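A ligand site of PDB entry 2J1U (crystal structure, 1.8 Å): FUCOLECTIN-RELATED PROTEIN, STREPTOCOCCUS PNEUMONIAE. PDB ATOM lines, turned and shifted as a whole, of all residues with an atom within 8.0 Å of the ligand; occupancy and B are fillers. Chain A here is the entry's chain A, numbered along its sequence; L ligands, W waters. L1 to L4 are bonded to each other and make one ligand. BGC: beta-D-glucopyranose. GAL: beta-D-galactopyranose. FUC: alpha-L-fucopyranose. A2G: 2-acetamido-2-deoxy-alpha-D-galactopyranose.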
ATOM      1  N   ASP A  30      10.687 -16.195   9.437  1.00  0.00           N
ATOM      2  CA  ASP A  30      11.756 -15.471   8.806  1.00  0.00           C
ATOM      3  C   ASP A  30      11.190 -14.847   7.527  1.00  0.00           C
ATOM      4  O   ASP A  30      10.247 -15.378   6.898  1.00  0.00           O
ATOM      5  CB  ASP A  30      12.932 -16.411   8.447  1.00  0.00           C
ATOM      6  CG  ASP A  30      14.273 -15.739   8.528  1.00  0.00           C
ATOM      7  OD1 ASP A  30      14.341 -14.510   8.758  1.00  0.00           O
ATOM      8  OD2 ASP A  30      15.344 -16.376   8.454  1.00  0.00           O
ATOM      9  N   TYR A  31      11.842 -13.758   7.112  1.00  0.00           N
ATOM     10  CA  TYR A  31      11.492 -13.006   5.898  1.00  0.00           C
ATOM     11  C   TYR A  31      10.036 -12.681   5.788  1.00  0.00           C
ATOM     12  O   TYR A  31       9.462 -12.709   4.687  1.00  0.00           O
ATOM     13  CB  TYR A  31      11.933 -13.778   4.675  1.00  0.00           C
ATOM     14  CG  TYR A  31      13.411 -14.191   4.720  1.00  0.00           C
ATOM     15  CD1 TYR A  31      13.766 -15.519   4.873  1.00  0.00           C
ATOM     16  CD2 TYR A  31      14.425 -13.269   4.553  1.00  0.00           C
ATOM     17  CE1 TYR A  31      15.099 -15.916   4.893  1.00  0.00           C
ATOM     18  CE2 TYR A  31      15.784 -13.664   4.556  1.00  0.00           C
ATOM     19  CZ  TYR A  31      16.098 -14.978   4.736  1.00  0.00           C
ATOM     20  OH  TYR A  31      17.391 -15.424   4.777  1.00  0.00           O
ATOM     21  N   PHE A  47       8.093 -17.094  -3.647  1.00  0.00           N
ATOM     22  CA  PHE A  47       8.176 -16.502  -2.332  1.00  0.00           C
ATOM     23  C   PHE A  47       8.092 -14.972  -2.351  1.00  0.00           C
ATOM     24  O   PHE A  47       7.498 -14.334  -1.495  1.00  0.00           O
ATOM     25  CB  PHE A  47       9.493 -16.898  -1.617  1.00  0.00           C
ATOM     26  CG  PHE A  47       9.603 -16.295  -0.282  1.00  0.00           C
ATOM     27  CD1 PHE A  47      10.333 -15.155  -0.066  1.00  0.00           C
ATOM     28  CD2 PHE A  47       8.912 -16.830   0.755  1.00  0.00           C
ATOM     29  CE1 PHE A  47      10.365 -14.576   1.171  1.00  0.00           C
ATOM     30  CE2 PHE A  47       8.910 -16.204   2.014  1.00  0.00           C
ATOM     31  CZ  PHE A  47       9.650 -15.097   2.193  1.00  0.00           C
ATOM     32  N   ASN A  48       8.701 -14.364  -3.369  1.00  0.00           N
ATOM     33  CA  ASN A  48       8.834 -12.933  -3.446  1.00  0.00           C
ATOM     34  C   ASN A  48       7.508 -12.212  -3.730  1.00  0.00           C
ATOM     35  O   ASN A  48       7.381 -11.018  -3.531  1.00  0.00           O
ATOM     36  CB  ASN A  48       9.898 -12.571  -4.466  1.00  0.00           C
ATOM     37  CG  ASN A  48      11.265 -13.154  -4.078  1.00  0.00           C
ATOM     38  OD1 ASN A  48      11.871 -12.726  -3.103  1.00  0.00           O
ATOM     39  ND2 ASN A  48      11.699 -14.169  -4.812  1.00  0.00           N
ATOM     40  N   THR A  53       4.956 -19.212   3.042  1.00  0.00           N
ATOM     41  CA  THR A  53       5.465 -19.124   4.384  1.00  0.00           C
ATOM     42  C   THR A  53       6.997 -19.322   4.390  1.00  0.00           C
ATOM     43  O   THR A  53       7.585 -19.807   3.425  1.00  0.00           O
ATOM     44  CB  THR A  53       4.852 -20.191   5.282  1.00  0.00           C
ATOM     45  OG1 THR A  53       5.279 -21.507   4.863  1.00  0.00           O
ATOM     46  CG2 THR A  53       3.308 -20.212   5.219  1.00  0.00           C
ATOM     47  N   HIS A  54       7.593 -19.041   5.554  1.00  0.00           N
ATOM     48  CA  HIS A  54       9.016 -19.251   5.760  1.00  0.00           C
ATOM     49  C   HIS A  54       9.307 -19.258   7.238  1.00  0.00           C
ATOM     50  O   HIS A  54       9.029 -18.306   7.918  1.00  0.00           O
ATOM     51  CB  HIS A  54       9.788 -18.129   5.078  1.00  0.00           C
ATOM     52  CG  HIS A  54      11.154 -18.495   4.620  1.00  0.00           C
ATOM     53  ND1 HIS A  54      12.179 -18.825   5.484  1.00  0.00           N
ATOM     54  CD2 HIS A  54      11.687 -18.499   3.377  1.00  0.00           C
ATOM     55  CE1 HIS A  54      13.275 -19.055   4.772  1.00  0.00           C
ATOM     56  NE2 HIS A  54      13.011 -18.864   3.494  1.00  0.00           N
ATOM     57  N   THR A  55       9.853 -20.366   7.741  1.00  0.00           N
ATOM     58  CA  THR A  55      10.355 -20.397   9.139  1.00  0.00           C
ATOM     59  C   THR A  55      11.872 -20.071   9.119  1.00  0.00           C
ATOM     60  O   THR A  55      12.449 -19.937   8.039  1.00  0.00           O
ATOM     61  CB  THR A  55      10.090 -21.758   9.814  1.00  0.00           C
ATOM     62  OG1 THR A  55      10.984 -22.783   9.279  1.00  0.00           O
ATOM     63  CG2 THR A  55       8.659 -22.257   9.584  1.00  0.00           C
ATOM     64  N   ARG A  81       6.933 -24.140  -2.374  1.00  0.00           N
ATOM     65  CA  ARG A  81       7.628 -23.008  -2.923  1.00  0.00           C
ATOM     66  C   ARG A  81       8.121 -23.470  -4.289  1.00  0.00           C
ATOM     67  O   ARG A  81       8.481 -24.650  -4.475  1.00  0.00           O
ATOM     68  CB  ARG A  81       8.816 -22.662  -2.063  1.00  0.00           C
ATOM     69  CG  ARG A  81       9.466 -21.374  -2.473  1.00  0.00           C
ATOM     70  CD  ARG A  81      10.617 -20.931  -1.545  1.00  0.00           C
ATOM     71  NE  ARG A  81      11.343 -19.829  -2.162  1.00  0.00           N
ATOM     72  CZ  ARG A  81      12.403 -19.225  -1.623  1.00  0.00           C
ATOM     73  NH1 ARG A  81      12.900 -19.644  -0.467  1.00  0.00           N
ATOM     74  NH2 ARG A  81      13.016 -18.247  -2.274  1.00  0.00           N
ATOM     75  N   THR A  82       8.133 -22.548  -5.240  1.00  0.00           N
ATOM     76  CA  THR A  82       8.496 -22.889  -6.627  1.00  0.00           C
ATOM     77  C   THR A  82       9.636 -22.014  -7.182  1.00  0.00           C
ATOM     78  O   THR A  82      10.295 -22.430  -8.159  1.00  0.00           O
ATOM     79  CB  THR A  82       7.256 -22.825  -7.553  1.00  0.00           C
ATOM     80  OG1 THR A  82       6.643 -21.511  -7.528  1.00  0.00           O
ATOM     81  CG2 THR A  82       6.163 -23.840  -7.111  1.00  0.00           C
ATOM     82  N   ASP A  83       9.888 -20.829  -6.611  1.00  0.00           N
ATOM     83  CA  ASP A  83      10.890 -19.972  -7.212  1.00  0.00           C
ATOM     84  C   ASP A  83      12.336 -20.443  -6.912  1.00  0.00           C
ATOM     85  O   ASP A  83      13.282 -20.220  -7.713  1.00  0.00           O
ATOM     86  CB  ASP A  83      10.740 -18.524  -6.803  1.00  0.00           C
ATOM     87  CG  ASP A  83      10.934 -18.318  -5.340  1.00  0.00           C
ATOM     88  OD1 ASP A  83      11.928 -17.638  -4.992  1.00  0.00           O
ATOM     89  OD2 ASP A  83      10.144 -18.806  -4.493  1.00  0.00           O
ATOM     90  N   ALA A  84      12.497 -21.111  -5.785  1.00  0.00           N
ATOM     91  CA  ALA A  84      13.830 -21.496  -5.305  1.00  0.00           C
ATOM     92  C   ALA A  84      13.706 -22.530  -4.178  1.00  0.00           C
ATOM     93  O   ALA A  84      12.690 -22.603  -3.531  1.00  0.00           O
ATOM     94  CB  ALA A  84      14.502 -20.349  -4.743  1.00  0.00           C
ATOM     95  N   GLU A  85      14.798 -23.264  -3.936  1.00  0.00           N
ATOM     96  CA  GLU A  85      14.957 -24.104  -2.740  1.00  0.00           C
ATOM     97  C   GLU A  85      13.812 -25.127  -2.573  1.00  0.00           C
ATOM     98  O   GLU A  85      13.420 -25.492  -1.453  1.00  0.00           O
ATOM     99  CB  GLU A  85      15.114 -23.233  -1.518  1.00  0.00           C
ATOM    100  CG  GLU A  85      16.253 -22.254  -1.548  1.00  0.00           C
ATOM    101  CD  GLU A  85      17.618 -22.828  -1.214  1.00  0.00           C
ATOM    102  OE1 GLU A  85      17.792 -24.076  -1.188  1.00  0.00           O
ATOM    103  OE2 GLU A  85      18.510 -21.966  -0.951  1.00  0.00           O
ATOM    104  N   THR A  86      13.343 -25.655  -3.713  1.00  0.00           N
ATOM    105  CA  THR A  86      12.221 -26.573  -3.719  1.00  0.00           C
ATOM    106  C   THR A  86      12.496 -27.862  -2.960  1.00  0.00           C
ATOM    107  O   THR A  86      11.589 -28.440  -2.377  1.00  0.00           O
ATOM    108  CB  THR A  86      11.726 -26.854  -5.117  1.00  0.00           C
ATOM    109  OG1 THR A  86      12.717 -27.541  -5.882  1.00  0.00           O
ATOM    110  CG2 THR A  86      11.453 -25.541  -5.873  1.00  0.00           C
ATOM    111  N   GLN A  87      13.773 -28.276  -2.925  1.00  0.00           N
ATOM    112  CA  GLN A  87      14.147 -29.483  -2.265  1.00  0.00           C
ATOM    113  C   GLN A  87      14.027 -29.387  -0.743  1.00  0.00           C
ATOM    114  O   GLN A  87      14.102 -30.421  -0.036  1.00  0.00           O
ATOM    115  CB  GLN A  87      15.567 -29.896  -2.668  1.00  0.00           C
ATOM    116  CG  GLN A  87      16.633 -29.210  -1.861  1.00  0.00           C
ATOM    117  CD  GLN A  87      16.715 -27.683  -2.046  1.00  0.00           C
ATOM    118  OE1 GLN A  87      16.456 -27.155  -3.158  1.00  0.00           O
ATOM    119  NE2 GLN A  87      17.097 -26.998  -0.979  1.00  0.00           N
ATOM    120  N   ARG A  88      13.793 -28.184  -0.204  1.00  0.00           N
ATOM    121  CA  ARG A  88      13.610 -28.060   1.223  1.00  0.00           C
ATOM    122  C   ARG A  88      12.384 -28.855   1.685  1.00  0.00           C
ATOM    123  O   ARG A  88      12.366 -29.346   2.816  1.00  0.00           O
ATOM    124  CB  ARG A  88      13.482 -26.602   1.638  1.00  0.00           C
ATOM    125  CG  ARG A  88      14.783 -25.847   1.625  1.00  0.00           C
ATOM    126  CD  ARG A  88      14.656 -24.397   2.063  1.00  0.00           C
ATOM    127  NE  ARG A  88      15.999 -23.841   2.196  1.00  0.00           N
ATOM    128  CZ  ARG A  88      16.267 -22.532   2.261  1.00  0.00           C
ATOM    129  NH1 ARG A  88      15.275 -21.629   2.211  1.00  0.00           N
ATOM    130  NH2 ARG A  88      17.500 -22.129   2.363  1.00  0.00           N
ATOM    131  N   PRO A 139      14.773 -24.418   6.694  1.00  0.00           N
ATOM    132  CA  PRO A 139      13.522 -23.665   6.735  1.00  0.00           C
ATOM    133  C   PRO A 139      12.389 -24.381   6.017  1.00  0.00           C
ATOM    134  O   PRO A 139      12.620 -25.023   5.011  1.00  0.00           O
ATOM    135  CB  PRO A 139      13.856 -22.387   5.947  1.00  0.00           C
ATOM    136  CG  PRO A 139      15.235 -22.245   6.046  1.00  0.00           C
ATOM    137  CD  PRO A 139      15.824 -23.661   5.998  1.00  0.00           C
ATOM    138  N   SER A 141       9.010 -23.769   3.986  1.00  0.00           N
ATOM    139  CA  SER A 141       8.175 -22.862   3.197  1.00  0.00           C
ATOM    140  C   SER A 141       7.081 -23.623   2.441  1.00  0.00           C
ATOM    141  O   SER A 141       7.304 -24.627   1.713  1.00  0.00           O
ATOM    142  CB  SER A 141       9.019 -22.040   2.181  1.00  0.00           C
ATOM    143  OG  SER A 141       9.940 -21.220   2.863  1.00  0.00           O
HETATM  144  C2  BGC L   1      15.910 -10.823   0.677  1.00  0.00           C
HETATM  145  C3  BGC L   1      15.872 -12.057  -0.214  1.00  0.00           C
HETATM  146  C4  BGC L   1      17.119 -12.915  -0.065  1.00  0.00           C
HETATM  147  C5  BGC L   1      17.360 -13.204   1.423  1.00  0.00           C
HETATM  148  C6  BGC L   1      18.645 -13.981   1.692  1.00  0.00           C
HETATM  149  C1  BGC L   1      16.148 -11.258   2.118  1.00  0.00           C
HETATM  150  O1  BGC L   1      16.261 -10.130   2.966  1.00  0.00           O
HETATM  151  O2  BGC L   1      14.701 -10.134   0.612  1.00  0.00           O
HETATM  152  O3  BGC L   1      15.835 -11.631  -1.544  1.00  0.00           O
HETATM  153  O4  BGC L   1      16.970 -14.090  -0.880  1.00  0.00           O
HETATM  154  O5  BGC L   1      17.331 -12.012   2.193  1.00  0.00           O
HETATM  155  O6  BGC L   1      19.809 -13.304   1.268  1.00  0.00           O
HETATM  156  C1  GAL L   2      18.074 -14.352  -1.719  1.00  0.00           C
HETATM  157  C2  GAL L   2      17.880 -15.797  -2.224  1.00  0.00           C
HETATM  158  C3  GAL L   2      19.056 -16.143  -3.116  1.00  0.00           C
HETATM  159  C4  GAL L   2      19.271 -15.110  -4.222  1.00  0.00           C
HETATM  160  C5  GAL L   2      19.422 -13.754  -3.576  1.00  0.00           C
HETATM  161  C6  GAL L   2      19.684 -12.678  -4.636  1.00  0.00           C
HETATM  162  O2  GAL L   2      17.833 -16.737  -1.122  1.00  0.00           O
HETATM  163  O3  GAL L   2      18.797 -17.401  -3.667  1.00  0.00           O
HETATM  164  O4  GAL L   2      18.179 -15.091  -5.119  1.00  0.00           O
HETATM  165  O5  GAL L   2      18.230 -13.435  -2.834  1.00  0.00           O
HETATM  166  O6  GAL L   2      19.942 -11.470  -3.972  1.00  0.00           O
HETATM  167  C1  FUC L   3      16.789 -17.691  -1.174  1.00  0.00           C
HETATM  168  C2  FUC L   3      17.211 -18.739  -0.121  1.00  0.00           C
HETATM  169  C3  FUC L   3      17.079 -18.179   1.291  1.00  0.00           C
HETATM  170  C4  FUC L   3      15.629 -17.689   1.476  1.00  0.00           C
HETATM  171  C5  FUC L   3      15.342 -16.591   0.435  1.00  0.00           C
HETATM  172  C6  FUC L   3      13.965 -15.894   0.619  1.00  0.00           C
HETATM  173  O2  FUC L   3      18.506 -19.256  -0.344  1.00  0.00           O
HETATM  174  O3  FUC L   3      17.428 -19.186   2.237  1.00  0.00           O
HETATM  175  O4  FUC L   3      14.765 -18.788   1.400  1.00  0.00           O
HETATM  176  O5  FUC L   3      15.492 -17.177  -0.874  1.00  0.00           O
HETATM  177  O5  A2G L   4      20.978 -18.112  -3.865  1.00  0.00           O
HETATM  178  C1  A2G L   4      19.679 -18.033  -4.469  1.00  0.00           C
HETATM  179  C2  A2G L   4      19.301 -19.386  -5.041  1.00  0.00           C
HETATM  180  N2  A2G L   4      18.002 -19.167  -5.754  1.00  0.00           N
HETATM  181  C3  A2G L   4      19.256 -20.388  -3.887  1.00  0.00           C
HETATM  182  O3  A2G L   4      18.892 -21.706  -4.332  1.00  0.00           O
HETATM  183  C4  A2G L   4      20.597 -20.451  -3.164  1.00  0.00           C
HETATM  184  O4  A2G L   4      21.587 -20.951  -4.075  1.00  0.00           O
HETATM  185  C5  A2G L   4      21.007 -19.036  -2.733  1.00  0.00           C
HETATM  186  C6  A2G L   4      22.393 -18.948  -2.084  1.00  0.00           C
HETATM  187  O6  A2G L   4      22.419 -19.593  -0.782  1.00  0.00           O
HETATM  188  C7  A2G L   4      17.673 -19.573  -6.991  1.00  0.00           C
HETATM  189  O7  A2G L   4      16.602 -19.360  -7.611  1.00  0.00           O
HETATM  190  C8  A2G L   4      18.689 -20.352  -7.624  1.00  0.00           C
HETATM  191  O   HOH W   1      18.720  -9.584   3.336  1.00  0.00           O
HETATM  192  O   HOH W   2      19.078 -15.322  -7.622  1.00  0.00           O
HETATM  193  O   HOH W   3      19.660 -24.684  -2.733  1.00  0.00           O
HETATM  194  O   HOH W   4      18.022 -18.038   4.545  1.00  0.00           O
HETATM  195  O   HOH W   5      16.000 -17.087  -4.998  1.00  0.00           O
HETATM  196  O   HOH W   6      15.078 -13.368  -3.928  1.00  0.00           O
HETATM  197  O   HOH W   7      16.763 -22.749  -5.906  1.00  0.00           O
HETATM  198  O   HOH W   8      21.232 -11.853   3.557  1.00  0.00           O
HETATM  199  O   HOH W   9      22.666 -23.010  -2.769  1.00  0.00           O
HETATM  200  O   HOH W  10      21.040 -15.337  -0.088  1.00  0.00           O
HETATM  201  O   HOH W  11      20.681 -18.044   0.676  1.00  0.00           O
HETATM  202  O   HOH W  12      23.129 -11.276  -4.037  1.00  0.00           O
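O4 of FUC L3 sits at hydrogen-bond distance from NE2 of His 54, 2.7 Å away.
The guanidinium group (NH1) of Arg 81 lies within hydrogen-bond range of an oxygen (O4) of FUC L3, at 2.8 Å.
An oxygen (O2) of FUC L3 lies within hydrogen-bond range of the side-chain carboxylate (OE2) of Glu 85 (2.8 Å).
O3 of FUC L3 sits at hydrogen-bond distance from NH2 of Arg 88.
O of His 54 is in hydrogen-bond range of N of Asp 30.
NE of Arg 81 lies within salt-bridge range of OD2 of Asp 83, 2.8 Å away.
The guanidinium group (NE) of Arg 81 sits close to the backbone carbonyl oxygen (O) of Ala 84.
The guanidinium group of Arg 88 lies within salt-bridge range of the side-chain carboxylate of Glu 85 (3.5 Å).
NE2 of Gln 87 is in hydrogen-bond range of OE1 of Glu 85 (3.0 Å).
The side-chain carboxylate (OD2) of Asp 83 is in hydrogen-bond range of the backbone NH (N) of Phe 47, 2.8 Å away.
The side-chain carboxylate of Asp 83 is in hydrogen-bond range of the side-chain amide nitrogen of Asn 48.
O of Asp 83 sits close to O7 of A2G L4 (3.4 Å).
Tyr 31 touches the ligand.
CD1 of Phe 47 touches C6 of FUC L3 (3.8 Å).
CB of Ala 84 touches O7 of A2G L4, at 3.7 Å.
Hydrophobic or aromatic side chains within 4 Å of the ligand: Tyr 31, Phe 47, His 54 and Ala 84.
Water W4 lies within hydrogen-bond range of an oxygen (O3) of FUC L3 (2.6 Å) and the side-chain hydroxyl of Tyr 31 (2.7 Å).
Water W7 lies within hydrogen-bond range of the backbone NH of Glu 85 (2.8 Å) and an oxygen (O3) of A2G L4 (2.8 Å).
Water W6 bridges an oxygen (O3) of BGC L1 (3.0 Å) and the side-chain amide oxygen (OD1) of Asn 48 (3.4 Å).
Water W3 bridges the side-chain carboxylate of Glu 85 (2.5 Å) and an oxygen (O3) of A2G L4 (3.5 Å).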
